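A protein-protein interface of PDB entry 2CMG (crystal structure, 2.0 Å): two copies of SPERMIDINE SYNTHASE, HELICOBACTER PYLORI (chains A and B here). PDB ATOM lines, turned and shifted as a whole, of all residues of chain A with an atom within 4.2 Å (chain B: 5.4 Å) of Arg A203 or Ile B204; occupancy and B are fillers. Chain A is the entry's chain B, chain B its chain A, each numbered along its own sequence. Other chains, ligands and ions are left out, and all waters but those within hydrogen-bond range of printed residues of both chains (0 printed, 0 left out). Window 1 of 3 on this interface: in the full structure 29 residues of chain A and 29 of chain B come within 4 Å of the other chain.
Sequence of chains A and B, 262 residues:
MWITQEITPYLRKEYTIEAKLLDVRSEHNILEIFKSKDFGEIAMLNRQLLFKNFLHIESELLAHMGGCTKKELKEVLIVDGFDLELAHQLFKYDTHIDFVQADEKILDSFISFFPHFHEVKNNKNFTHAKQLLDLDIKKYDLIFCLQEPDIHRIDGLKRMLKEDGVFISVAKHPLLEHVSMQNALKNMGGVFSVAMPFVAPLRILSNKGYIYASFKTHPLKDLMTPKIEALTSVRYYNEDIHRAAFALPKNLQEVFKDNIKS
O of Ile B204 sits close to O of Ile A204, at 2.6 Å.
Printed residues of chain B within 4 Å of His A173: Leu B202 and Ile B204. Pro A201 touches none of the printed residues of chain B. Of the printed residues of chain B, Leu A202 touches His B173 and Leu B175. Arg A203 touches one residue of chain B. Ser A206 touches none of the printed residues of chain B. Of the printed residues of chain A, Leu B175 touches Leu A202. Printed residues of chain A within 4 Å of Leu B202: His A173 (3.1 Å). Of the printed residues of chain A, Arg B203 touches Ile A204 (3.8 Å). Of chain A, only His A173 (3.3 Å), Arg A203 (3.5 Å) and Ile A204 (2.6 Å) come within 4 Å of Ile B204. The nearest residue of chain B that does not touch Arg A203 is Leu B175 (4.8 Å).
Of the 9 printed residues of chain A, 4 touch a printed residue of chain B. Printed residues of chain A that touch a printed residue of chain B: His A173, Leu A202, Arg A203 and Ile A204. Hydrophobic or aromatic side chains of chain A within 4 Å of the printed part of chain B: His A173, Leu A202 and Ile A204. Of the 7 printed residues of chain B, 5 touch a printed residue of chain A. Printed residues of chain B that touch a printed residue of chain A: His B173, Leu B175, Leu B202, Arg B203 and Ile B204. Hydrophobic or aromatic side chains of chain B that line the printed part of chain A: His B173, Leu B175, Leu B202 and Ile B204. Among the printed residues, 8 pairs touch across the chains. Among the printed residues, no Asp or Glu carboxylate lies within 4 Å of a Lys or Arg side-chain nitrogen of the other chain.
Among the printed residues, pairs that only touch across the chains: Ile A204 with His B173 (2.9 Å), Leu A202 with Leu B175 (3.0 Å), His A173 with Leu B202 (3.1 Å), Leu A202 with His B173 (3.3 Å), His A173 with Ile B204 (3.3 Å), Arg A203 with Ile B204 (3.5 Å) and Ile A204 with Arg B203 (3.8 Å).
His A173 touches Leu B202, and with the chains exchanged Leu A202 touches His B173. His A173 touches Ile B204, and with the chains exchanged Ile A204 touches His B173. Arg A203 touches Ile B204, and with the chains exchanged Ile A204 touches Arg B203. Ile A204 touches its own counterpart, Ile B204. 6 positions are printed for both chains. Of the 8 pairs that touch across the chains among the printed residues, 7 have their exchanged pair printed and touching as well.
The backbone carbonyl oxygen (O) of Arg B203 sits at hydrogen-bond distance from the side-chain hydroxyl (OG) of Ser B206 (3.3 Å). NH2 of Arg A203 lies within hydrogen-bond range of OG of Ser A206, 2.6 Å away.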
ATOM      1  N   ILE A  57       4.974 -15.588  -8.288  1.00  0.00           N
ATOM      2  CA  ILE A  57       5.104 -14.145  -8.097  1.00  0.00           C
ATOM      3  C   ILE A  57       6.481 -13.652  -7.659  1.00  0.00           C
ATOM      4  O   ILE A  57       7.176 -12.963  -8.408  1.00  0.00           O
ATOM      5  CB  ILE A  57       4.021 -13.575  -7.122  1.00  0.00           C
ATOM      6  CG1 ILE A  57       3.738 -14.514  -5.937  1.00  0.00           C
ATOM      7  CG2 ILE A  57       2.709 -13.396  -7.889  1.00  0.00           C
ATOM      8  CD1 ILE A  57       4.711 -14.431  -4.789  1.00  0.00           C
ATOM      9  N   HIS A 173       7.786  -4.921   5.077  1.00  0.00           N
ATOM     10  CA  HIS A 173       6.963  -4.036   4.253  1.00  0.00           C
ATOM     11  C   HIS A 173       7.242  -2.627   4.737  1.00  0.00           C
ATOM     12  O   HIS A 173       7.109  -2.347   5.923  1.00  0.00           O
ATOM     13  CB  HIS A 173       5.470  -4.336   4.408  1.00  0.00           C
ATOM     14  CG  HIS A 173       4.629  -3.692   3.350  1.00  0.00           C
ATOM     15  ND1 HIS A 173       4.040  -2.458   3.510  1.00  0.00           N
ATOM     16  CD2 HIS A 173       4.353  -4.077   2.083  1.00  0.00           C
ATOM     17  CE1 HIS A 173       3.439  -2.108   2.388  1.00  0.00           C
ATOM     18  NE2 HIS A 173       3.615  -3.076   1.504  1.00  0.00           N
ATOM     19  N   ALA A 200       6.294  -6.366  -3.932  1.00  0.00           N
ATOM     20  CA  ALA A 200       5.667  -7.127  -5.004  1.00  0.00           C
ATOM     21  C   ALA A 200       4.265  -6.548  -5.204  1.00  0.00           C
ATOM     22  O   ALA A 200       3.361  -6.782  -4.407  1.00  0.00           O
ATOM     23  CB  ALA A 200       5.593  -8.602  -4.635  1.00  0.00           C
ATOM     24  N   PRO A 201       4.077  -5.754  -6.263  1.00  0.00           N
ATOM     25  CA  PRO A 201       2.755  -5.177  -6.495  1.00  0.00           C
ATOM     26  C   PRO A 201       1.649  -6.231  -6.502  1.00  0.00           C
ATOM     27  O   PRO A 201       1.816  -7.334  -7.034  1.00  0.00           O
ATOM     28  CB  PRO A 201       2.925  -4.481  -7.838  1.00  0.00           C
ATOM     29  CG  PRO A 201       4.339  -3.986  -7.751  1.00  0.00           C
ATOM     30  CD  PRO A 201       5.061  -5.210  -7.217  1.00  0.00           C
ATOM     31  N   LEU A 202       0.526  -5.872  -5.889  1.00  0.00           N
ATOM     32  CA  LEU A 202      -0.641  -6.734  -5.797  1.00  0.00           C
ATOM     33  C   LEU A 202      -0.552  -7.842  -4.761  1.00  0.00           C
ATOM     34  O   LEU A 202      -1.541  -8.533  -4.516  1.00  0.00           O
ATOM     35  CB  LEU A 202      -0.975  -7.337  -7.160  1.00  0.00           C
ATOM     36  CG  LEU A 202      -1.541  -6.376  -8.202  1.00  0.00           C
ATOM     37  CD1 LEU A 202      -2.785  -5.728  -7.620  1.00  0.00           C
ATOM     38  CD2 LEU A 202      -0.498  -5.324  -8.604  1.00  0.00           C
ATOM     39  N   ARG A 203       0.616  -8.030  -4.150  1.00  0.00           N
ATOM     40  CA  ARG A 203       0.725  -9.069  -3.132  1.00  0.00           C
ATOM     41  C   ARG A 203       0.256  -8.440  -1.827  1.00  0.00           C
ATOM     42  O   ARG A 203       0.948  -7.616  -1.224  1.00  0.00           O
ATOM     43  CB  ARG A 203       2.163  -9.586  -3.028  1.00  0.00           C
ATOM     44  CG  ARG A 203       2.234 -11.078  -2.686  1.00  0.00           C
ATOM     45  CD  ARG A 203       3.662 -11.611  -2.677  1.00  0.00           C
ATOM     46  NE  ARG A 203       3.708 -13.043  -2.409  1.00  0.00           N
ATOM     47  CZ  ARG A 203       4.028 -13.577  -1.234  1.00  0.00           C
ATOM     48  NH1 ARG A 203       4.038 -14.895  -1.083  1.00  0.00           N
ATOM     49  NH2 ARG A 203       4.355 -12.795  -0.216  1.00  0.00           N
ATOM     50  N   ILE A 204      -0.945  -8.827  -1.410  1.00  0.00           N
ATOM     51  CA  ILE A 204      -1.567  -8.277  -0.216  1.00  0.00           C
ATOM     52  C   ILE A 204      -1.577  -9.185   1.006  1.00  0.00           C
ATOM     53  O   ILE A 204      -1.970  -8.752   2.091  1.00  0.00           O
ATOM     54  CB  ILE A 204      -3.012  -7.844  -0.526  1.00  0.00           C
ATOM     55  CG1 ILE A 204      -3.705  -8.926  -1.364  1.00  0.00           C
ATOM     56  CG2 ILE A 204      -3.015  -6.494  -1.242  1.00  0.00           C
ATOM     57  CD1 ILE A 204      -5.224  -8.844  -1.357  1.00  0.00           C
ATOM     58  N   LEU A 205      -1.153 -10.433   0.849  1.00  0.00           N
ATOM     59  CA  LEU A 205      -1.114 -11.338   1.993  1.00  0.00           C
ATOM     60  C   LEU A 205       0.295 -11.586   2.554  1.00  0.00           C
ATOM     61  O   LEU A 205       0.713 -12.738   2.719  1.00  0.00           O
ATOM     62  CB  LEU A 205      -1.785 -12.670   1.637  1.00  0.00           C
ATOM     63  CG  LEU A 205      -1.450 -13.410   0.335  1.00  0.00           C
ATOM     64  CD1 LEU A 205       0.006 -13.826   0.302  1.00  0.00           C
ATOM     65  CD2 LEU A 205      -2.354 -14.636   0.232  1.00  0.00           C
ATOM     66  N   SER A 206       1.021 -10.510   2.855  1.00  0.00           N
ATOM     67  CA  SER A 206       2.374 -10.660   3.401  1.00  0.00           C
ATOM     68  C   SER A 206       3.135  -9.376   3.711  1.00  0.00           C
ATOM     69  O   SER A 206       3.272  -8.489   2.870  1.00  0.00           O
ATOM     70  CB  SER A 206       3.236 -11.515   2.468  1.00  0.00           C
ATOM     71  OG  SER A 206       3.455 -10.855   1.233  1.00  0.00           O
ATOM     72  N   HIS B 173     -10.531  -7.258  -4.922  1.00  0.00           N
ATOM     73  CA  HIS B 173      -9.115  -7.293  -5.258  1.00  0.00           C
ATOM     74  C   HIS B 173      -8.996  -8.368  -6.336  1.00  0.00           C
ATOM     75  O   HIS B 173      -9.456  -9.500  -6.154  1.00  0.00           O
ATOM     76  CB  HIS B 173      -8.264  -7.668  -4.036  1.00  0.00           C
ATOM     77  CG  HIS B 173      -6.828  -7.263  -4.163  1.00  0.00           C
ATOM     78  ND1 HIS B 173      -5.790  -8.171  -4.170  1.00  0.00           N
ATOM     79  CD2 HIS B 173      -6.263  -6.043  -4.324  1.00  0.00           C
ATOM     80  CE1 HIS B 173      -4.648  -7.526  -4.333  1.00  0.00           C
ATOM     81  NE2 HIS B 173      -4.907  -6.234  -4.429  1.00  0.00           N
ATOM     82  N   LEU B 175      -6.432  -9.942  -7.260  1.00  0.00           N
ATOM     83  CA  LEU B 175      -5.395 -10.916  -6.936  1.00  0.00           C
ATOM     84  C   LEU B 175      -6.044 -12.236  -6.534  1.00  0.00           C
ATOM     85  O   LEU B 175      -5.755 -13.285  -7.103  1.00  0.00           O
ATOM     86  CB  LEU B 175      -4.509 -10.372  -5.798  1.00  0.00           C
ATOM     87  CG  LEU B 175      -3.113 -10.903  -5.457  1.00  0.00           C
ATOM     88  CD1 LEU B 175      -3.212 -12.124  -4.557  1.00  0.00           C
ATOM     89  CD2 LEU B 175      -2.351 -11.221  -6.732  1.00  0.00           C
ATOM     90  N   LEU B 202       0.797  -0.571  -1.910  1.00  0.00           N
ATOM     91  CA  LEU B 202       1.307  -0.725  -0.557  1.00  0.00           C
ATOM     92  C   LEU B 202       0.257  -0.985   0.523  1.00  0.00           C
ATOM     93  O   LEU B 202       0.600  -1.146   1.689  1.00  0.00           O
ATOM     94  CB  LEU B 202       2.160   0.499  -0.176  1.00  0.00           C
ATOM     95  CG  LEU B 202       3.478   0.704  -0.946  1.00  0.00           C
ATOM     96  CD1 LEU B 202       3.232   1.521  -2.209  1.00  0.00           C
ATOM     97  CD2 LEU B 202       4.487   1.408  -0.043  1.00  0.00           C
ATOM     98  N   ARG B 203      -1.014  -1.034   0.144  1.00  0.00           N
ATOM     99  CA  ARG B 203      -2.081  -1.300   1.111  1.00  0.00           C
ATOM    100  C   ARG B 203      -2.325  -2.796   1.244  1.00  0.00           C
ATOM    101  O   ARG B 203      -3.342  -3.321   0.781  1.00  0.00           O
ATOM    102  CB  ARG B 203      -3.370  -0.601   0.693  1.00  0.00           C
ATOM    103  CG  ARG B 203      -3.583   0.733   1.363  1.00  0.00           C
ATOM    104  CD  ARG B 203      -4.954   1.298   1.048  1.00  0.00           C
ATOM    105  NE  ARG B 203      -6.054   0.567   1.674  1.00  0.00           N
ATOM    106  CZ  ARG B 203      -6.601   0.895   2.844  1.00  0.00           C
ATOM    107  NH1 ARG B 203      -7.601   0.181   3.347  1.00  0.00           N
ATOM    108  NH2 ARG B 203      -6.144   1.940   3.518  1.00  0.00           N
ATOM    109  N   ILE B 204      -1.386  -3.482   1.884  1.00  0.00           N
ATOM    110  CA  ILE B 204      -1.485  -4.922   2.043  1.00  0.00           C
ATOM    111  C   ILE B 204      -2.634  -5.349   2.938  1.00  0.00           C
ATOM    112  O   ILE B 204      -2.978  -6.528   2.991  1.00  0.00           O
ATOM    113  CB  ILE B 204      -0.142  -5.545   2.574  1.00  0.00           C
ATOM    114  CG1 ILE B 204       0.314  -4.869   3.877  1.00  0.00           C
ATOM    115  CG2 ILE B 204       0.944  -5.428   1.507  1.00  0.00           C
ATOM    116  CD1 ILE B 204       0.706  -3.370   3.823  1.00  0.00           C
ATOM    117  N   LEU B 205      -3.240  -4.390   3.626  1.00  0.00           N
ATOM    118  CA  LEU B 205      -4.367  -4.693   4.506  1.00  0.00           C
ATOM    119  C   LEU B 205      -5.738  -4.393   3.898  1.00  0.00           C
ATOM    120  O   LEU B 205      -6.643  -3.964   4.608  1.00  0.00           O
ATOM    121  CB  LEU B 205      -4.222  -3.945   5.835  1.00  0.00           C
ATOM    122  CG  LEU B 205      -3.034  -4.321   6.741  1.00  0.00           C
ATOM    123  CD1 LEU B 205      -2.956  -5.834   6.879  1.00  0.00           C
ATOM    124  CD2 LEU B 205      -1.728  -3.787   6.169  1.00  0.00           C
ATOM    125  N   SER B 206      -5.899  -4.630   2.597  1.00  0.00           N
ATOM    126  CA  SER B 206      -7.193  -4.385   1.954  1.00  0.00           C
ATOM    127  C   SER B 206      -7.503  -5.251   0.730  1.00  0.00           C
ATOM    128  O   SER B 206      -6.787  -5.222  -0.277  1.00  0.00           O
ATOM    129  CB  SER B 206      -7.321  -2.911   1.559  1.00  0.00           C
ATOM    130  OG  SER B 206      -6.511  -2.609   0.443  1.00  0.00           O
